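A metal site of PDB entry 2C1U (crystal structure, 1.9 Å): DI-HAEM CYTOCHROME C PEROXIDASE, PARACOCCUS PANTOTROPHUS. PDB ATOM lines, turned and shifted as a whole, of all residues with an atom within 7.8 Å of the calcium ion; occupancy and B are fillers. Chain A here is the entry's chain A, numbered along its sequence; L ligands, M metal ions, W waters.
N of Phe 274 lies within hydrogen-bond range of O2 of the ligand. N of His 275 lies within hydrogen-bond range of O3 of the ligand (2.6 Å). O4 of the ligand lies within hydrogen-bond range of ND1 of His 275, 2.7 Å away.
The side-chain hydroxyl (OG1) of Thr 270 is in hydrogen-bond range of the backbone carbonyl oxygen (O) of Val 267, at 3.4 Å. NE1 of Trp 108 sits at hydrogen-bond distance from O of Asn 93 (2.6 Å). The side-chain amide nitrogen (ND2) of Asn 93 is in hydrogen-bond range of the backbone carbonyl oxygen (O) of Leu 79, 2.9 Å away. The side-chain amide nitrogen of Asn 93 lies within hydrogen-bond range of the backbone carbonyl oxygen of Pro 80, 3.0 Å away. O of His 275 lies within hydrogen-bond range of N of Asn 93.
The nearest printed residue that does not touch the calcium ion is Ala 271 (4.3 Å).
The calcium ion is bound by water W3 (2.3 Å), the backbone carbonyl oxygen (O) of Thr 270 (2.4 Å), the side-chain amide oxygen (OD1) of Asn 93 (2.4 Å), the backbone carbonyl oxygen (O) of Pro 272 (2.4 Å), water W4 (2.4 Å), water W2 (2.5 Å) and water W1 (2.6 Å). The calcium ion has seven donor atoms within binding distance.
Water W4 bridges O2 of the ligand (3.0 Å) and N of Phe 274 (3.4 Å). Water W2 bridges the side-chain hydroxyl (OG1) of Thr 270 (2.6 Å) and an oxygen (O1) of the ligand (2.7 Å). Water W1 lies within hydrogen-bond range of the backbone carbonyl oxygen of Ala 271 (3.1 Å) and the side-chain amide nitrogen of Asn 93 (3.2 Å).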
ATOM      1  N   VAL A  76      30.605  -6.790  -6.835  1.00  0.00           N
ATOM      2  CA  VAL A  76      30.377  -6.508  -5.429  1.00  0.00           C
ATOM      3  C   VAL A  76      31.517  -7.093  -4.609  1.00  0.00           C
ATOM      4  O   VAL A  76      32.319  -7.830  -5.141  1.00  0.00           O
ATOM      5  CB  VAL A  76      28.980  -7.075  -4.902  1.00  0.00           C
ATOM      6  CG1 VAL A  76      27.809  -6.479  -5.684  1.00  0.00           C
ATOM      7  CG2 VAL A  76      28.919  -8.614  -4.904  1.00  0.00           C
ATOM      8  N   ASP A  77      31.583  -6.819  -3.317  1.00  0.00           N
ATOM      9  CA  ASP A  77      32.733  -7.356  -2.551  1.00  0.00           C
ATOM     10  C   ASP A  77      32.324  -8.616  -1.764  1.00  0.00           C
ATOM     11  O   ASP A  77      33.173  -9.295  -1.186  1.00  0.00           O
ATOM     12  CB  ASP A  77      33.340  -6.281  -1.621  1.00  0.00           C
ATOM     13  CG  ASP A  77      32.342  -5.707  -0.603  1.00  0.00           C
ATOM     14  OD1 ASP A  77      31.193  -6.233  -0.450  1.00  0.00           O
ATOM     15  OD2 ASP A  77      32.616  -4.665   0.090  1.00  0.00           O
ATOM     16  N   GLY A  78      31.029  -8.957  -1.750  1.00  0.00           N
ATOM     17  CA  GLY A  78      30.545 -10.173  -1.035  1.00  0.00           C
ATOM     18  C   GLY A  78      30.640 -10.062   0.484  1.00  0.00           C
ATOM     19  O   GLY A  78      30.767 -11.087   1.217  1.00  0.00           O
ATOM     20  N   LEU A  79      30.619  -8.815   0.983  1.00  0.00           N
ATOM     21  CA  LEU A  79      30.691  -8.545   2.441  1.00  0.00           C
ATOM     22  C   LEU A  79      29.434  -7.779   2.927  1.00  0.00           C
ATOM     23  O   LEU A  79      28.813  -7.107   2.143  1.00  0.00           O
ATOM     24  CB  LEU A  79      31.947  -7.758   2.778  1.00  0.00           C
ATOM     25  CG  LEU A  79      33.254  -8.432   2.340  1.00  0.00           C
ATOM     26  CD1 LEU A  79      34.395  -7.575   2.825  1.00  0.00           C
ATOM     27  CD2 LEU A  79      33.417  -9.809   2.914  1.00  0.00           C
ATOM     28  N   PRO A  80      29.064  -7.895   4.198  1.00  0.00           N
ATOM     29  CA  PRO A  80      27.854  -7.233   4.690  1.00  0.00           C
ATOM     30  C   PRO A  80      27.790  -5.722   4.400  1.00  0.00           C
ATOM     31  O   PRO A  80      26.880  -5.295   3.732  1.00  0.00           O
ATOM     32  CB  PRO A  80      27.832  -7.546   6.182  1.00  0.00           C
ATOM     33  CG  PRO A  80      28.659  -8.806   6.309  1.00  0.00           C
ATOM     34  CD  PRO A  80      29.719  -8.711   5.245  1.00  0.00           C
ATOM     35  N   ASN A  93      25.520  -2.318   2.266  1.00  0.00           N
ATOM     36  CA  ASN A  93      25.956  -3.362   1.372  1.00  0.00           C
ATOM     37  C   ASN A  93      26.247  -2.745   0.006  1.00  0.00           C
ATOM     38  O   ASN A  93      25.393  -2.017  -0.564  1.00  0.00           O
ATOM     39  CB  ASN A  93      24.829  -4.397   1.241  1.00  0.00           C
ATOM     40  CG  ASN A  93      25.259  -5.603   0.480  1.00  0.00           C
ATOM     41  OD1 ASN A  93      24.798  -5.861  -0.606  1.00  0.00           O
ATOM     42  ND2 ASN A  93      26.214  -6.315   1.045  1.00  0.00           N
ATOM     43  N   ALA A  94      27.424  -3.036  -0.549  1.00  0.00           N
ATOM     44  CA  ALA A  94      27.766  -2.502  -1.863  1.00  0.00           C
ATOM     45  C   ALA A  94      26.899  -3.125  -2.957  1.00  0.00           C
ATOM     46  O   ALA A  94      26.841  -4.350  -3.059  1.00  0.00           O
ATOM     47  CB  ALA A  94      29.220  -2.764  -2.149  1.00  0.00           C
ATOM     48  N   PRO A  95      26.171  -2.297  -3.718  1.00  0.00           N
ATOM     49  CA  PRO A  95      25.400  -2.780  -4.858  1.00  0.00           C
ATOM     50  C   PRO A  95      26.344  -3.146  -6.001  1.00  0.00           C
ATOM     51  O   PRO A  95      27.458  -2.616  -6.103  1.00  0.00           O
ATOM     52  CB  PRO A  95      24.520  -1.579  -5.248  1.00  0.00           C
ATOM     53  CG  PRO A  95      25.278  -0.409  -4.839  1.00  0.00           C
ATOM     54  CD  PRO A  95      26.030  -0.839  -3.560  1.00  0.00           C
ATOM     55  N   THR A  96      25.910  -4.052  -6.872  1.00  0.00           N
ATOM     56  CA  THR A  96      26.703  -4.394  -8.019  1.00  0.00           C
ATOM     57  C   THR A  96      26.872  -3.231  -9.027  1.00  0.00           C
ATOM     58  O   THR A  96      25.905  -2.497  -9.350  1.00  0.00           O
ATOM     59  CB  THR A  96      26.106  -5.655  -8.716  1.00  0.00           C
ATOM     60  OG1 THR A  96      26.982  -6.071  -9.773  1.00  0.00           O
ATOM     61  CG2 THR A  96      24.752  -5.350  -9.442  1.00  0.00           C
ATOM     62  N   TRP A 108      20.719   3.530  -2.097  1.00  0.00           N
ATOM     63  CA  TRP A 108      19.989   2.532  -1.322  1.00  0.00           C
ATOM     64  C   TRP A 108      18.783   3.129  -0.649  1.00  0.00           C
ATOM     65  O   TRP A 108      17.740   2.531  -0.664  1.00  0.00           O
ATOM     66  CB  TRP A 108      20.852   1.894  -0.218  1.00  0.00           C
ATOM     67  CG  TRP A 108      21.456   0.556  -0.555  1.00  0.00           C
ATOM     68  CD1 TRP A 108      22.784   0.253  -0.674  1.00  0.00           C
ATOM     69  CD2 TRP A 108      20.746  -0.677  -0.793  1.00  0.00           C
ATOM     70  NE1 TRP A 108      22.954  -1.093  -0.954  1.00  0.00           N
ATOM     71  CE2 TRP A 108      21.718  -1.678  -1.032  1.00  0.00           C
ATOM     72  CE3 TRP A 108      19.384  -1.030  -0.796  1.00  0.00           C
ATOM     73  CZ2 TRP A 108      21.372  -3.005  -1.312  1.00  0.00           C
ATOM     74  CZ3 TRP A 108      19.045  -2.369  -1.073  1.00  0.00           C
ATOM     75  CH2 TRP A 108      20.030  -3.332  -1.311  1.00  0.00           C
ATOM     76  N   VAL A 267      21.424 -11.402  -9.057  1.00  0.00           N
ATOM     77  CA  VAL A 267      21.199 -11.546  -7.595  1.00  0.00           C
ATOM     78  C   VAL A 267      21.834 -12.798  -7.035  1.00  0.00           C
ATOM     79  O   VAL A 267      22.325 -12.773  -5.911  1.00  0.00           O
ATOM     80  CB  VAL A 267      19.691 -11.396  -7.136  1.00  0.00           C
ATOM     81  CG1 VAL A 267      18.750 -12.468  -7.733  1.00  0.00           C
ATOM     82  CG2 VAL A 267      19.566 -11.355  -5.577  1.00  0.00           C
ATOM     83  N   LEU A 269      24.594 -13.871  -7.694  1.00  0.00           N
ATOM     84  CA  LEU A 269      26.029 -13.602  -7.526  1.00  0.00           C
ATOM     85  C   LEU A 269      26.335 -12.635  -6.391  1.00  0.00           C
ATOM     86  O   LEU A 269      27.512 -12.519  -5.956  1.00  0.00           O
ATOM     87  CB  LEU A 269      26.638 -13.035  -8.830  1.00  0.00           C
ATOM     88  CG  LEU A 269      26.339 -13.786 -10.143  1.00  0.00           C
ATOM     89  CD1 LEU A 269      27.230 -13.319 -11.291  1.00  0.00           C
ATOM     90  CD2 LEU A 269      26.438 -15.284  -9.961  1.00  0.00           C
ATOM     91  N   THR A 270      25.321 -11.956  -5.884  1.00  0.00           N
ATOM     92  CA  THR A 270      25.618 -10.784  -5.039  1.00  0.00           C
ATOM     93  C   THR A 270      25.199 -10.816  -3.593  1.00  0.00           C
ATOM     94  O   THR A 270      24.881  -9.757  -3.023  1.00  0.00           O
ATOM     95  CB  THR A 270      25.063  -9.511  -5.697  1.00  0.00           C
ATOM     96  OG1 THR A 270      23.642  -9.628  -5.770  1.00  0.00           O
ATOM     97  CG2 THR A 270      25.529  -9.471  -7.166  1.00  0.00           C
ATOM     98  N   ALA A 271      25.245 -12.007  -2.982  1.00  0.00           N
ATOM     99  CA  ALA A 271      25.001 -12.118  -1.549  1.00  0.00           C
ATOM    100  C   ALA A 271      26.116 -11.372  -0.850  1.00  0.00           C
ATOM    101  O   ALA A 271      27.177 -11.220  -1.433  1.00  0.00           O
ATOM    102  CB  ALA A 271      24.987 -13.573  -1.108  1.00  0.00           C
ATOM    103  N   PRO A 272      25.908 -10.951   0.397  1.00  0.00           N
ATOM    104  CA  PRO A 272      24.631 -11.024   1.096  1.00  0.00           C
ATOM    105  C   PRO A 272      23.569  -9.979   0.685  1.00  0.00           C
ATOM    106  O   PRO A 272      23.820  -9.111  -0.145  1.00  0.00           O
ATOM    107  CB  PRO A 272      25.064 -10.845   2.564  1.00  0.00           C
ATOM    108  CG  PRO A 272      26.207  -9.787   2.462  1.00  0.00           C
ATOM    109  CD  PRO A 272      26.889 -10.124   1.128  1.00  0.00           C
ATOM    110  N   TYR A 273      22.363 -10.099   1.221  1.00  0.00           N
ATOM    111  CA  TYR A 273      21.215  -9.365   0.631  1.00  0.00           C
ATOM    112  C   TYR A 273      20.702  -8.289   1.580  1.00  0.00           C
ATOM    113  O   TYR A 273      21.050  -8.285   2.794  1.00  0.00           O
ATOM    114  CB  TYR A 273      20.125 -10.336   0.206  1.00  0.00           C
ATOM    115  CG  TYR A 273      20.656 -11.341  -0.782  1.00  0.00           C
ATOM    116  CD1 TYR A 273      21.017 -10.935  -2.095  1.00  0.00           C
ATOM    117  CD2 TYR A 273      20.919 -12.662  -0.398  1.00  0.00           C
ATOM    118  CE1 TYR A 273      21.536 -11.835  -2.995  1.00  0.00           C
ATOM    119  CE2 TYR A 273      21.462 -13.584  -1.303  1.00  0.00           C
ATOM    120  CZ  TYR A 273      21.789 -13.148  -2.593  1.00  0.00           C
ATOM    121  OH  TYR A 273      22.317 -14.052  -3.492  1.00  0.00           O
ATOM    122  N   PHE A 274      19.936  -7.379   0.995  1.00  0.00           N
ATOM    123  CA  PHE A 274      19.353  -6.185   1.615  1.00  0.00           C
ATOM    124  C   PHE A 274      20.372  -5.086   1.916  1.00  0.00           C
ATOM    125  O   PHE A 274      21.623  -5.342   1.909  1.00  0.00           O
ATOM    126  CB  PHE A 274      18.484  -6.578   2.825  1.00  0.00           C
ATOM    127  CG  PHE A 274      17.377  -7.552   2.452  1.00  0.00           C
ATOM    128  CD1 PHE A 274      16.283  -7.126   1.682  1.00  0.00           C
ATOM    129  CD2 PHE A 274      17.465  -8.895   2.792  1.00  0.00           C
ATOM    130  CE1 PHE A 274      15.294  -8.018   1.287  1.00  0.00           C
ATOM    131  CE2 PHE A 274      16.468  -9.808   2.392  1.00  0.00           C
ATOM    132  CZ  PHE A 274      15.372  -9.355   1.636  1.00  0.00           C
ATOM    133  N   HIS A 275      19.865  -3.896   2.248  1.00  0.00           N
ATOM    134  CA  HIS A 275      20.733  -2.723   2.356  1.00  0.00           C
ATOM    135  C   HIS A 275      21.822  -2.919   3.418  1.00  0.00           C
ATOM    136  O   HIS A 275      22.846  -2.241   3.372  1.00  0.00           O
ATOM    137  CB  HIS A 275      19.900  -1.463   2.693  1.00  0.00           C
ATOM    138  CG  HIS A 275      19.317  -1.494   4.068  1.00  0.00           C
ATOM    139  ND1 HIS A 275      18.132  -2.145   4.366  1.00  0.00           N
ATOM    140  CD2 HIS A 275      19.770  -0.971   5.232  1.00  0.00           C
ATOM    141  CE1 HIS A 275      17.880  -2.013   5.666  1.00  0.00           C
ATOM    142  NE2 HIS A 275      18.858  -1.299   6.209  1.00  0.00           N
ATOM    143  N   GLY A 277      23.045  -6.105   4.340  1.00  0.00           N
ATOM    144  CA  GLY A 277      23.830  -7.299   3.976  1.00  0.00           C
ATOM    145  C   GLY A 277      23.839  -8.360   5.080  1.00  0.00           C
ATOM    146  O   GLY A 277      24.875  -8.996   5.377  1.00  0.00           O
ATOM    147  N   VAL A 279      21.373 -11.014   5.237  1.00  0.00           N
ATOM    148  CA  VAL A 279      20.767 -12.275   4.787  1.00  0.00           C
ATOM    149  C   VAL A 279      21.711 -12.937   3.772  1.00  0.00           C
ATOM    150  O   VAL A 279      22.047 -12.329   2.738  1.00  0.00           O
ATOM    151  CB  VAL A 279      19.364 -12.033   4.129  1.00  0.00           C
ATOM    152  CG1 VAL A 279      18.804 -13.321   3.511  1.00  0.00           C
ATOM    153  CG2 VAL A 279      18.358 -11.415   5.177  1.00  0.00           C
HETATM  154 FE1  LIG L   1      11.681  -6.865  -3.247  1.00  0.00          FE
HETATM  155  C1  LIG L   1      14.871  -6.216  -2.044  1.00  0.00           C
HETATM  156  C2  LIG L   1      12.749 -10.122  -3.987  1.00  0.00           C
HETATM  157  C3  LIG L   1       8.592  -7.684  -3.973  1.00  0.00           C
HETATM  158  C4  LIG L   1      10.772  -3.564  -2.828  1.00  0.00           C
HETATM  159  N1  LIG L   1      13.488  -7.961  -3.045  1.00  0.00           N
HETATM  160  C5  LIG L   1      14.683  -7.488  -2.566  1.00  0.00           C
HETATM  161  C6  LIG L   1      15.668  -8.568  -2.662  1.00  0.00           C
HETATM  162  C7  LIG L   1      15.074  -9.636  -3.201  1.00  0.00           C
HETATM  163  C8  LIG L   1      13.703  -9.270  -3.458  1.00  0.00           C
HETATM  164  C9  LIG L   1      15.679 -11.026  -3.524  1.00  0.00           C
HETATM  165  C10 LIG L   1      17.158  -8.471  -2.224  1.00  0.00           C
HETATM  166  C11 LIG L   1      17.974  -8.148  -3.489  1.00  0.00           C
HETATM  167  C12 LIG L   1      19.321  -7.600  -3.092  1.00  0.00           C
HETATM  168  O1  LIG L   1      20.134  -7.264  -4.009  1.00  0.00           O
HETATM  169  O2  LIG L   1      19.568  -7.493  -1.883  1.00  0.00           O
HETATM  170  N2  LIG L   1      10.890  -8.558  -3.853  1.00  0.00           N
HETATM  171  C13 LIG L   1      11.424  -9.805  -4.109  1.00  0.00           C
HETATM  172  C14 LIG L   1      10.358 -10.714  -4.427  1.00  0.00           C
HETATM  173  C15 LIG L   1       9.221 -10.034  -4.487  1.00  0.00           C
HETATM  174  C16 LIG L   1       9.523  -8.678  -4.069  1.00  0.00           C
HETATM  175  C17 LIG L   1      10.549 -12.184  -4.860  1.00  0.00           C
HETATM  176  C18 LIG L   1       7.808 -10.600  -4.796  1.00  0.00           C
HETATM  177  C19 LIG L   1       7.524 -11.803  -3.859  1.00  0.00           C
HETATM  178  N3  LIG L   1       9.987  -5.798  -3.390  1.00  0.00           N
HETATM  179  C20 LIG L   1       8.780  -6.355  -3.703  1.00  0.00           C
HETATM  180  C21 LIG L   1       7.774  -5.310  -3.774  1.00  0.00           C
HETATM  181  C22 LIG L   1       8.358  -4.157  -3.390  1.00  0.00           C
HETATM  182  C23 LIG L   1       9.773  -4.443  -3.185  1.00  0.00           C
HETATM  183  C24 LIG L   1       6.253  -5.504  -3.991  1.00  0.00           C
HETATM  184  C25 LIG L   1       7.706  -2.748  -3.319  1.00  0.00           C
HETATM  185  C26 LIG L   1       6.784  -2.491  -2.139  1.00  0.00           C
HETATM  186  N4  LIG L   1      12.648  -5.169  -2.580  1.00  0.00           N
HETATM  187  C27 LIG L   1      12.035  -3.950  -2.379  1.00  0.00           C
HETATM  188  C28 LIG L   1      12.938  -3.100  -1.632  1.00  0.00           C
HETATM  189  C29 LIG L   1      14.196  -3.928  -1.371  1.00  0.00           C
HETATM  190  C30 LIG L   1      13.948  -5.191  -2.029  1.00  0.00           C
HETATM  191  C31 LIG L   1      12.648  -1.659  -1.159  1.00  0.00           C
HETATM  192  C32 LIG L   1      15.485  -3.507  -0.570  1.00  0.00           C
HETATM  193  C33 LIG L   1      15.084  -3.602   0.912  1.00  0.00           C
HETATM  194  C34 LIG L   1      16.259  -3.459   1.878  1.00  0.00           C
HETATM  195  O3  LIG L   1      17.420  -3.646   1.451  1.00  0.00           O
HETATM  196  O4  LIG L   1      16.045  -3.214   3.076  1.00  0.00           O
HETATM  197 CA    CA M   1      24.275  -7.708  -2.021  1.00  0.00          CA
HETATM  198  O   HOH W   1      26.762  -8.119  -1.535  1.00  0.00           O
HETATM  199  O   HOH W   2      22.603  -8.362  -3.699  1.00  0.00           O
HETATM  200  O   HOH W   3      24.804  -6.259  -3.693  1.00  0.00           O
HETATM  201  O   HOH W   4      22.313  -6.516  -1.348  1.00  0.00           O
